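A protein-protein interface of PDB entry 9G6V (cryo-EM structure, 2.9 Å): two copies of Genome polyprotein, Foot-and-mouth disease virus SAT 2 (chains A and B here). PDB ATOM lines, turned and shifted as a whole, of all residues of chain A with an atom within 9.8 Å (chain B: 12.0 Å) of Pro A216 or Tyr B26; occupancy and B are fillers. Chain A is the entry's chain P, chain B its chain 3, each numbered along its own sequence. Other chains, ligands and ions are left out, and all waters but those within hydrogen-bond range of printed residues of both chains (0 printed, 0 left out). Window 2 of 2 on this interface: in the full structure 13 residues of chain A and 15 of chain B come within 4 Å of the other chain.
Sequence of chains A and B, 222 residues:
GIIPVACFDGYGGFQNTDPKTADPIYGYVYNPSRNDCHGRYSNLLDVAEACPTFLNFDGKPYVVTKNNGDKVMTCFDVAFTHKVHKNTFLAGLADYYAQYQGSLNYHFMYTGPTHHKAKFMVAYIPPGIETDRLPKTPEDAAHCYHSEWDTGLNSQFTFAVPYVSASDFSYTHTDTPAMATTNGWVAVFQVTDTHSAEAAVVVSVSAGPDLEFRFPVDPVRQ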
ATOM      1  N   GLN A  15      43.605  20.390  19.434  1.00  0.00           N
ATOM      2  CA  GLN A  15      42.170  20.160  19.480  1.00  0.00           C
ATOM      3  C   GLN A  15      41.498  21.296  20.235  1.00  0.00           C
ATOM      4  O   GLN A  15      41.974  21.722  21.291  1.00  0.00           O
ATOM      5  CB  GLN A  15      41.850  18.831  20.161  1.00  0.00           C
ATOM      6  CG  GLN A  15      42.532  17.631  19.550  1.00  0.00           C
ATOM      7  CD  GLN A  15      42.064  16.335  20.173  1.00  0.00           C
ATOM      8  OE1 GLN A  15      41.172  16.330  21.021  1.00  0.00           O
ATOM      9  NE2 GLN A  15      42.664  15.225  19.755  1.00  0.00           N
ATOM     10  N   ASN A  16      40.389  21.787  19.688  1.00  0.00           N
ATOM     11  CA  ASN A  16      39.669  22.869  20.344  1.00  0.00           C
ATOM     12  C   ASN A  16      38.775  22.384  21.476  1.00  0.00           C
ATOM     13  O   ASN A  16      38.208  23.214  22.193  1.00  0.00           O
ATOM     14  CB  ASN A  16      38.837  23.644  19.322  1.00  0.00           C
ATOM     15  CG  ASN A  16      37.688  22.836  18.775  1.00  0.00           C
ATOM     16  OD1 ASN A  16      37.738  21.609  18.745  1.00  0.00           O
ATOM     17  ND2 ASN A  16      36.641  23.521  18.337  1.00  0.00           N
ATOM     18  N   THR A  17      38.633  21.069  21.656  1.00  0.00           N
ATOM     19  CA  THR A  17      37.811  20.503  22.720  1.00  0.00           C
ATOM     20  C   THR A  17      38.595  19.484  23.538  1.00  0.00           C
ATOM     21  O   THR A  17      38.014  18.548  24.092  1.00  0.00           O
ATOM     22  CB  THR A  17      36.546  19.860  22.153  1.00  0.00           C
ATOM     23  OG1 THR A  17      36.908  18.784  21.279  1.00  0.00           O
ATOM     24  CG2 THR A  17      35.726  20.877  21.379  1.00  0.00           C
ATOM     25  N   ASP A  18      39.911  19.647  23.621  1.00  0.00           N
ATOM     26  CA  ASP A  18      40.732  18.679  24.330  1.00  0.00           C
ATOM     27  C   ASP A  18      40.519  18.801  25.838  1.00  0.00           C
ATOM     28  O   ASP A  18      40.357  19.909  26.358  1.00  0.00           O
ATOM     29  CB  ASP A  18      42.209  18.877  23.993  1.00  0.00           C
ATOM     30  CG  ASP A  18      42.640  20.325  24.093  1.00  0.00           C
ATOM     31  OD1 ASP A  18      41.771  21.193  24.310  1.00  0.00           O
ATOM     32  OD2 ASP A  18      43.851  20.597  23.952  1.00  0.00           O
ATOM     33  N   PRO A  19      40.508  17.682  26.566  1.00  0.00           N
ATOM     34  CA  PRO A  19      40.348  17.760  28.027  1.00  0.00           C
ATOM     35  C   PRO A  19      41.572  18.296  28.746  1.00  0.00           C
ATOM     36  O   PRO A  19      41.457  18.691  29.913  1.00  0.00           O
ATOM     37  CB  PRO A  19      40.062  16.306  28.431  1.00  0.00           C
ATOM     38  CG  PRO A  19      39.716  15.595  27.151  1.00  0.00           C
ATOM     39  CD  PRO A  19      40.491  16.293  26.086  1.00  0.00           C
ATOM     40  N   LEU A  44      21.870  24.640  31.631  1.00  0.00           N
ATOM     41  CA  LEU A  44      21.016  25.444  30.764  1.00  0.00           C
ATOM     42  C   LEU A  44      19.576  24.952  30.779  1.00  0.00           C
ATOM     43  O   LEU A  44      18.641  25.759  30.803  1.00  0.00           O
ATOM     44  CB  LEU A  44      21.567  25.443  29.341  1.00  0.00           C
ATOM     45  CG  LEU A  44      22.874  26.204  29.141  1.00  0.00           C
ATOM     46  CD1 LEU A  44      23.448  25.906  27.775  1.00  0.00           C
ATOM     47  CD2 LEU A  44      22.638  27.693  29.311  1.00  0.00           C
ATOM     48  N   LEU A  93      17.729  27.719  22.591  1.00  0.00           N
ATOM     49  CA  LEU A  93      18.643  26.740  23.164  1.00  0.00           C
ATOM     50  C   LEU A  93      18.804  25.526  22.260  1.00  0.00           C
ATOM     51  O   LEU A  93      19.879  24.919  22.225  1.00  0.00           O
ATOM     52  CB  LEU A  93      18.149  26.316  24.546  1.00  0.00           C
ATOM     53  CG  LEU A  93      19.064  25.390  25.344  1.00  0.00           C
ATOM     54  CD1 LEU A  93      20.394  26.068  25.611  1.00  0.00           C
ATOM     55  CD2 LEU A  93      18.397  24.979  26.643  1.00  0.00           C
ATOM     56  N   ALA A  94      17.754  25.158  21.523  1.00  0.00           N
ATOM     57  CA  ALA A  94      17.822  24.001  20.640  1.00  0.00           C
ATOM     58  C   ALA A  94      18.603  24.273  19.365  1.00  0.00           C
ATOM     59  O   ALA A  94      19.031  23.321  18.706  1.00  0.00           O
ATOM     60  CB  ALA A  94      16.415  23.532  20.274  1.00  0.00           C
ATOM     61  N   ASP A  95      18.789  25.541  18.998  1.00  0.00           N
ATOM     62  CA  ASP A  95      19.517  25.862  17.778  1.00  0.00           C
ATOM     63  C   ASP A  95      20.978  25.448  17.853  1.00  0.00           C
ATOM     64  O   ASP A  95      21.609  25.256  16.810  1.00  0.00           O
ATOM     65  CB  ASP A  95      19.418  27.358  17.484  1.00  0.00           C
ATOM     66  CG  ASP A  95      19.849  27.705  16.076  1.00  0.00           C
ATOM     67  OD1 ASP A  95      19.906  26.792  15.227  1.00  0.00           O
ATOM     68  OD2 ASP A  95      20.134  28.891  15.815  1.00  0.00           O
ATOM     69  N   TYR A  96      21.526  25.302  19.056  1.00  0.00           N
ATOM     70  CA  TYR A  96      22.929  24.968  19.239  1.00  0.00           C
ATOM     71  C   TYR A  96      23.148  23.501  19.580  1.00  0.00           C
ATOM     72  O   TYR A  96      24.276  23.115  19.899  1.00  0.00           O
ATOM     73  CB  TYR A  96      23.537  25.857  20.322  1.00  0.00           C
ATOM     74  CG  TYR A  96      23.417  27.327  20.008  1.00  0.00           C
ATOM     75  CD1 TYR A  96      24.352  27.962  19.205  1.00  0.00           C
ATOM     76  CD2 TYR A  96      22.360  28.077  20.498  1.00  0.00           C
ATOM     77  CE1 TYR A  96      24.242  29.301  18.906  1.00  0.00           C
ATOM     78  CE2 TYR A  96      22.242  29.417  20.204  1.00  0.00           C
ATOM     79  CZ  TYR A  96      23.185  30.024  19.407  1.00  0.00           C
ATOM     80  OH  TYR A  96      23.070  31.360  19.112  1.00  0.00           O
ATOM     81  N   TYR A  97      22.105  22.675  19.512  1.00  0.00           N
ATOM     82  CA  TYR A  97      22.204  21.258  19.825  1.00  0.00           C
ATOM     83  C   TYR A  97      21.650  20.432  18.676  1.00  0.00           C
ATOM     84  O   TYR A  97      20.618  20.775  18.093  1.00  0.00           O
ATOM     85  CB  TYR A  97      21.465  20.923  21.116  1.00  0.00           C
ATOM     86  CG  TYR A  97      22.189  21.396  22.349  1.00  0.00           C
ATOM     87  CD1 TYR A  97      23.225  20.656  22.891  1.00  0.00           C
ATOM     88  CD2 TYR A  97      21.842  22.586  22.968  1.00  0.00           C
ATOM     89  CE1 TYR A  97      23.894  21.081  24.012  1.00  0.00           C
ATOM     90  CE2 TYR A  97      22.506  23.019  24.091  1.00  0.00           C
ATOM     91  CZ  TYR A  97      23.531  22.261  24.608  1.00  0.00           C
ATOM     92  OH  TYR A  97      24.198  22.688  25.727  1.00  0.00           O
ATOM     93  N   ALA A  98      22.346  19.338  18.360  1.00  0.00           N
ATOM     94  CA  ALA A  98      21.975  18.520  17.211  1.00  0.00           C
ATOM     95  C   ALA A  98      20.712  17.709  17.480  1.00  0.00           C
ATOM     96  O   ALA A  98      19.814  17.647  16.635  1.00  0.00           O
ATOM     97  CB  ALA A  98      23.133  17.599  16.833  1.00  0.00           C
ATOM     98  N   GLN A  99      20.622  17.082  18.652  1.00  0.00           N
ATOM     99  CA  GLN A  99      19.560  16.132  18.949  1.00  0.00           C
ATOM    100  C   GLN A  99      18.950  16.431  20.311  1.00  0.00           C
ATOM    101  O   GLN A  99      19.532  17.135  21.141  1.00  0.00           O
ATOM    102  CB  GLN A  99      20.080  14.689  18.919  1.00  0.00           C
ATOM    103  CG  GLN A  99      20.666  14.267  17.588  1.00  0.00           C
ATOM    104  CD  GLN A  99      21.504  13.017  17.703  1.00  0.00           C
ATOM    105  OE1 GLN A  99      21.419  12.291  18.689  1.00  0.00           O
ATOM    106  NE2 GLN A  99      22.330  12.767  16.697  1.00  0.00           N
ATOM    107  N   TYR A 100      17.762  15.874  20.537  1.00  0.00           N
ATOM    108  CA  TYR A 100      17.062  16.041  21.804  1.00  0.00           C
ATOM    109  C   TYR A 100      16.097  14.881  21.997  1.00  0.00           C
ATOM    110  O   TYR A 100      15.773  14.150  21.060  1.00  0.00           O
ATOM    111  CB  TYR A 100      16.314  17.374  21.859  1.00  0.00           C
ATOM    112  CG  TYR A 100      14.981  17.384  21.149  1.00  0.00           C
ATOM    113  CD1 TYR A 100      14.896  17.680  19.800  1.00  0.00           C
ATOM    114  CD2 TYR A 100      13.805  17.117  21.836  1.00  0.00           C
ATOM    115  CE1 TYR A 100      13.684  17.701  19.152  1.00  0.00           C
ATOM    116  CE2 TYR A 100      12.590  17.132  21.196  1.00  0.00           C
ATOM    117  CZ  TYR A 100      12.535  17.425  19.855  1.00  0.00           C
ATOM    118  OH  TYR A 100      11.322  17.444  19.211  1.00  0.00           O
ATOM    119  N   THR A 172      16.875  18.402  16.121  1.00  0.00           N
ATOM    120  CA  THR A 172      16.394  19.750  16.402  1.00  0.00           C
ATOM    121  C   THR A 172      16.200  20.547  15.119  1.00  0.00           C
ATOM    122  O   THR A 172      15.228  21.300  14.991  1.00  0.00           O
ATOM    123  CB  THR A 172      17.364  20.470  17.334  1.00  0.00           C
ATOM    124  OG1 THR A 172      18.646  20.568  16.703  1.00  0.00           O
ATOM    125  CG2 THR A 172      17.513  19.706  18.632  1.00  0.00           C
ATOM    126  N   HIS A 173      17.109  20.393  14.158  1.00  0.00           N
ATOM    127  CA  HIS A 173      17.036  21.119  12.898  1.00  0.00           C
ATOM    128  C   HIS A 173      16.320  20.272  11.854  1.00  0.00           C
ATOM    129  O   HIS A 173      16.713  19.131  11.596  1.00  0.00           O
ATOM    130  CB  HIS A 173      18.435  21.485  12.399  1.00  0.00           C
ATOM    131  CG  HIS A 173      19.280  22.186  13.417  1.00  0.00           C
ATOM    132  ND1 HIS A 173      20.103  21.511  14.292  1.00  0.00           N
ATOM    133  CD2 HIS A 173      19.433  23.502  13.696  1.00  0.00           C
ATOM    134  CE1 HIS A 173      20.725  22.380  15.067  1.00  0.00           C
ATOM    135  NE2 HIS A 173      20.337  23.595  14.726  1.00  0.00           N
ATOM    136  N   PHE A 213      18.939  17.751  25.870  1.00  0.00           N
ATOM    137  CA  PHE A 213      19.656  18.061  24.644  1.00  0.00           C
ATOM    138  C   PHE A 213      21.032  17.405  24.667  1.00  0.00           C
ATOM    139  O   PHE A 213      21.555  17.040  25.722  1.00  0.00           O
ATOM    140  CB  PHE A 213      19.805  19.572  24.463  1.00  0.00           C
ATOM    141  CG  PHE A 213      18.528  20.274  24.113  1.00  0.00           C
ATOM    142  CD1 PHE A 213      18.008  20.196  22.839  1.00  0.00           C
ATOM    143  CD2 PHE A 213      17.861  21.034  25.053  1.00  0.00           C
ATOM    144  CE1 PHE A 213      16.838  20.845  22.513  1.00  0.00           C
ATOM    145  CE2 PHE A 213      16.691  21.688  24.730  1.00  0.00           C
ATOM    146  CZ  PHE A 213      16.180  21.592  23.459  1.00  0.00           C
ATOM    147  N   ARG A 214      21.623  17.265  23.484  1.00  0.00           N
ATOM    148  CA  ARG A 214      22.913  16.599  23.376  1.00  0.00           C
ATOM    149  C   ARG A 214      23.639  17.097  22.136  1.00  0.00           C
ATOM    150  O   ARG A 214      23.032  17.661  21.223  1.00  0.00           O
ATOM    151  CB  ARG A 214      22.747  15.080  23.321  1.00  0.00           C
ATOM    152  CG  ARG A 214      22.130  14.604  22.028  1.00  0.00           C
ATOM    153  CD  ARG A 214      21.817  13.125  22.058  1.00  0.00           C
ATOM    154  NE  ARG A 214      22.934  12.324  22.538  1.00  0.00           N
ATOM    155  CZ  ARG A 214      23.092  11.034  22.276  1.00  0.00           C
ATOM    156  NH1 ARG A 214      22.248  10.379  21.498  1.00  0.00           N
ATOM    157  NH2 ARG A 214      24.129  10.388  22.800  1.00  0.00           N
ATOM    158  N   PHE A 215      24.955  16.869  22.119  1.00  0.00           N
ATOM    159  CA  PHE A 215      25.816  17.159  20.977  1.00  0.00           C
ATOM    160  C   PHE A 215      25.760  18.630  20.593  1.00  0.00           C
ATOM    161  O   PHE A 215      25.142  18.980  19.581  1.00  0.00           O
ATOM    162  CB  PHE A 215      25.432  16.284  19.785  1.00  0.00           C
ATOM    163  CG  PHE A 215      25.546  14.818  20.057  1.00  0.00           C
ATOM    164  CD1 PHE A 215      26.552  14.333  20.871  1.00  0.00           C
ATOM    165  CD2 PHE A 215      24.642  13.928  19.516  1.00  0.00           C
ATOM    166  CE1 PHE A 215      26.659  12.989  21.133  1.00  0.00           C
ATOM    167  CE2 PHE A 215      24.743  12.583  19.779  1.00  0.00           C
ATOM    168  CZ  PHE A 215      25.756  12.112  20.585  1.00  0.00           C
ATOM    169  N   PRO A 216      26.368  19.516  21.379  1.00  0.00           N
ATOM    170  CA  PRO A 216      26.340  20.943  21.042  1.00  0.00           C
ATOM    171  C   PRO A 216      26.957  21.208  19.677  1.00  0.00           C
ATOM    172  O   PRO A 216      27.966  20.611  19.299  1.00  0.00           O
ATOM    173  CB  PRO A 216      27.156  21.588  22.167  1.00  0.00           C
ATOM    174  CG  PRO A 216      28.014  20.490  22.689  1.00  0.00           C
ATOM    175  CD  PRO A 216      27.197  19.245  22.565  1.00  0.00           C
ATOM    176  N   VAL A 217      26.335  22.122  18.939  1.00  0.00           N
ATOM    177  CA  VAL A 217      26.672  22.388  17.546  1.00  0.00           C
ATOM    178  C   VAL A 217      26.691  23.892  17.331  1.00  0.00           C
ATOM    179  O   VAL A 217      25.860  24.619  17.884  1.00  0.00           O
ATOM    180  CB  VAL A 217      25.666  21.708  16.592  1.00  0.00           C
ATOM    181  CG1 VAL A 217      25.815  22.229  15.176  1.00  0.00           C
ATOM    182  CG2 VAL A 217      25.849  20.209  16.614  1.00  0.00           C
ATOM    183  N   ASP A 218      27.649  24.365  16.536  1.00  0.00           N
ATOM    184  CA  ASP A 218      27.663  25.757  16.116  1.00  0.00           C
ATOM    185  C   ASP A 218      26.969  25.860  14.766  1.00  0.00           C
ATOM    186  O   ASP A 218      27.507  25.362  13.766  1.00  0.00           O
ATOM    187  CB  ASP A 218      29.086  26.276  16.026  1.00  0.00           C
ATOM    188  CG  ASP A 218      29.932  25.833  17.195  1.00  0.00           C
ATOM    189  OD1 ASP A 218      29.354  25.448  18.232  1.00  0.00           O
ATOM    190  OD2 ASP A 218      31.169  25.864  17.080  1.00  0.00           O
ATOM    191  N   PRO A 219      25.788  26.478  14.682  1.00  0.00           N
ATOM    192  CA  PRO A 219      25.097  26.602  13.391  1.00  0.00           C
ATOM    193  C   PRO A 219      25.751  27.683  12.542  1.00  0.00           C
ATOM    194  O   PRO A 219      25.875  28.832  12.970  1.00  0.00           O
ATOM    195  CB  PRO A 219      23.669  26.984  13.792  1.00  0.00           C
ATOM    196  CG  PRO A 219      23.833  27.689  15.095  1.00  0.00           C
ATOM    197  CD  PRO A 219      25.003  27.045  15.790  1.00  0.00           C
ATOM    198  N   ALA B  22      42.444   6.325  20.812  1.00  0.00           N
ATOM    199  CA  ALA B  22      42.579   7.714  20.400  1.00  0.00           C
ATOM    200  C   ALA B  22      41.938   8.632  21.437  1.00  0.00           C
ATOM    201  O   ALA B  22      41.359   8.186  22.430  1.00  0.00           O
ATOM    202  CB  ALA B  22      41.960   7.926  19.018  1.00  0.00           C
ATOM    203  N   ASP B  23      42.051   9.936  21.193  1.00  0.00           N
ATOM    204  CA  ASP B  23      41.494  10.933  22.096  1.00  0.00           C
ATOM    205  C   ASP B  23      40.092  11.309  21.639  1.00  0.00           C
ATOM    206  O   ASP B  23      39.938  11.852  20.536  1.00  0.00           O
ATOM    207  CB  ASP B  23      42.376  12.168  22.140  1.00  0.00           C
ATOM    208  CG  ASP B  23      43.787  11.859  22.596  1.00  0.00           C
ATOM    209  OD1 ASP B  23      44.068  10.681  22.907  1.00  0.00           O
ATOM    210  OD2 ASP B  23      44.617  12.791  22.645  1.00  0.00           O
ATOM    211  N   PRO B  24      39.057  11.051  22.434  1.00  0.00           N
ATOM    212  CA  PRO B  24      37.690  11.328  21.983  1.00  0.00           C
ATOM    213  C   PRO B  24      37.410  12.820  21.905  1.00  0.00           C
ATOM    214  O   PRO B  24      38.062  13.643  22.551  1.00  0.00           O
ATOM    215  CB  PRO B  24      36.823  10.656  23.051  1.00  0.00           C
ATOM    216  CG  PRO B  24      37.674  10.679  24.274  1.00  0.00           C
ATOM    217  CD  PRO B  24      39.092  10.509  23.803  1.00  0.00           C
ATOM    218  N   ILE B  25      36.415  13.161  21.090  1.00  0.00           N
ATOM    219  CA  ILE B  25      36.002  14.550  20.914  1.00  0.00           C
ATOM    220  C   ILE B  25      34.916  14.886  21.928  1.00  0.00           C
ATOM    221  O   ILE B  25      35.094  15.770  22.774  1.00  0.00           O
ATOM    222  CB  ILE B  25      35.520  14.806  19.477  1.00  0.00           C
ATOM    223  CG1 ILE B  25      36.700  14.754  18.505  1.00  0.00           C
ATOM    224  CG2 ILE B  25      34.806  16.138  19.393  1.00  0.00           C
ATOM    225  CD1 ILE B  25      36.327  15.062  17.076  1.00  0.00           C
ATOM    226  N   TYR B  26      33.786  14.189  21.851  1.00  0.00           N
ATOM    227  CA  TYR B  26      32.713  14.313  22.837  1.00  0.00           C
ATOM    228  C   TYR B  26      32.898  13.183  23.845  1.00  0.00           C
ATOM    229  O   TYR B  26      32.330  12.100  23.704  1.00  0.00           O
ATOM    230  CB  TYR B  26      31.342  14.255  22.175  1.00  0.00           C
ATOM    231  CG  TYR B  26      30.957  15.504  21.421  1.00  0.00           C
ATOM    232  CD1 TYR B  26      31.590  16.711  21.668  1.00  0.00           C
ATOM    233  CD2 TYR B  26      29.950  15.477  20.468  1.00  0.00           C
ATOM    234  CE1 TYR B  26      31.236  17.853  20.983  1.00  0.00           C
ATOM    235  CE2 TYR B  26      29.590  16.612  19.778  1.00  0.00           C
ATOM    236  CZ  TYR B  26      30.235  17.797  20.040  1.00  0.00           C
ATOM    237  OH  TYR B  26      29.880  18.934  19.354  1.00  0.00           O
ATOM    238  N   GLY B  27      33.699  13.443  24.875  1.00  0.00           N
ATOM    239  CA  GLY B  27      34.033  12.418  25.840  1.00  0.00           C
ATOM    240  C   GLY B  27      32.993  12.142  26.898  1.00  0.00           C
ATOM    241  O   GLY B  27      33.200  11.260  27.737  1.00  0.00           O
ATOM    242  N   TYR B  28      31.873  12.861  26.886  1.00  0.00           N
ATOM    243  CA  TYR B  28      30.852  12.686  27.911  1.00  0.00           C
ATOM    244  C   TYR B  28      29.525  12.250  27.305  1.00  0.00           C
ATOM    245  O   TYR B  28      28.469  12.780  27.665  1.00  0.00           O
ATOM    246  CB  TYR B  28      30.677  13.976  28.713  1.00  0.00           C
ATOM    247  CG  TYR B  28      31.825  14.264  29.653  1.00  0.00           C
ATOM    248  CD1 TYR B  28      32.990  14.867  29.197  1.00  0.00           C
ATOM    249  CD2 TYR B  28      31.744  13.929  30.999  1.00  0.00           C
ATOM    250  CE1 TYR B  28      34.043  15.127  30.053  1.00  0.00           C
ATOM    251  CE2 TYR B  28      32.790  14.187  31.862  1.00  0.00           C
ATOM    252  CZ  TYR B  28      33.936  14.786  31.385  1.00  0.00           C
ATOM    253  OH  TYR B  28      34.981  15.044  32.243  1.00  0.00           O
ATOM    254  N   VAL B  29      29.567  11.289  26.388  1.00  0.00           N
ATOM    255  CA  VAL B  29      28.363  10.725  25.789  1.00  0.00           C
ATOM    256  C   VAL B  29      28.036   9.421  26.500  1.00  0.00           C
ATOM    257  O   VAL B  29      28.925   8.706  26.979  1.00  0.00           O
ATOM    258  CB  VAL B  29      28.531  10.511  24.271  1.00  0.00           C
ATOM    259  CG1 VAL B  29      29.025  11.785  23.612  1.00  0.00           C
ATOM    260  CG2 VAL B  29      29.483   9.364  23.998  1.00  0.00           C
ATOM    261  N   TYR B  30      26.741   9.113  26.589  1.00  0.00           N
ATOM    262  CA  TYR B  30      26.269   7.912  27.285  1.00  0.00           C
ATOM    263  C   TYR B  30      25.079   7.350  26.509  1.00  0.00           C
ATOM    264  O   TYR B  30      23.938   7.771  26.713  1.00  0.00           O
ATOM    265  CB  TYR B  30      25.902   8.219  28.731  1.00  0.00           C
ATOM    266  CG  TYR B  30      26.987   8.939  29.499  1.00  0.00           C
ATOM    267  CD1 TYR B  30      28.068   8.246  30.027  1.00  0.00           C
ATOM    268  CD2 TYR B  30      26.928  10.312  29.696  1.00  0.00           C
ATOM    269  CE1 TYR B  30      29.062   8.903  30.728  1.00  0.00           C
ATOM    270  CE2 TYR B  30      27.916  10.977  30.396  1.00  0.00           C
ATOM    271  CZ  TYR B  30      28.980  10.268  30.910  1.00  0.00           C
ATOM    272  OH  TYR B  30      29.966  10.927  31.608  1.00  0.00           O
ATOM    273  N   ASN B  31      25.357   6.404  25.619  1.00  0.00           N
ATOM    274  CA  ASN B  31      24.283   5.716  24.920  1.00  0.00           C
ATOM    275  C   ASN B  31      23.523   4.823  25.900  1.00  0.00           C
ATOM    276  O   ASN B  31      24.139   4.169  26.748  1.00  0.00           O
ATOM    277  CB  ASN B  31      24.846   4.893  23.765  1.00  0.00           C
ATOM    278  CG  ASN B  31      25.712   5.723  22.837  1.00  0.00           C
ATOM    279  OD1 ASN B  31      25.206   6.456  21.988  1.00  0.00           O
ATOM    280  ND2 ASN B  31      27.025   5.617  23.000  1.00  0.00           N
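The side-chain hydroxyl of Tyr B26 lies within hydrogen-bond range of the backbone carbonyl oxygen of Pro A216 (2.5 Å).
The backbone NH (N) of Ala A98 sits at hydrogen-bond distance from the backbone carbonyl oxygen (O) of Phe A215.
Gln A15 touches Asp B23.
Thr A17 touches Ile B25.
Phe A215 touches Tyr B26.
Phe A215 touches Val B29 (CE1 to CG1, 3.6 Å).
Tyr B26 touches just these residues of chain A: Phe A215 (3.6 Å) and Pro A216 (2.5 Å).
Tyr A97 touches none of the printed residues of chain B.
Of chain B, only Tyr B26 and Val B29 come within 4 Å of Phe A215.
No residue of chain B comes within 4 Å of Asp A218.
Printed residues of chain A within 4 Å of Ile B25: Thr A17 (3.8 Å).
No residue of chain A comes within 4 Å of Gly B27.
Of the printed residues of chain B, Gln A15 touches Asp B23.
Of the printed residues of chain A, Val B29 touches Phe A215 (3.6 Å).
Ala A98 touches none of the printed residues of chain B.
Pro B24 touches none of the printed residues of chain A.
The nearest residue of chain A that does not touch Tyr B26 is Val A217 (4.8 Å).
Of the 10 printed residues of chain B, 4 touch a printed residue of chain A.
Hydrophobic or aromatic side chains of chain B within 4 Å of the printed part of chain A: Ile B25, Tyr B26 and Val B29.
Among the printed residues, no Asp or Glu carboxylate lies within 4 Å of a Lys or Arg side-chain nitrogen of the other chain.
No position is printed for both chains.
Of the 5 pairs that touch across the chains among the printed residues, none has its exchanged pair printed and touching as well.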
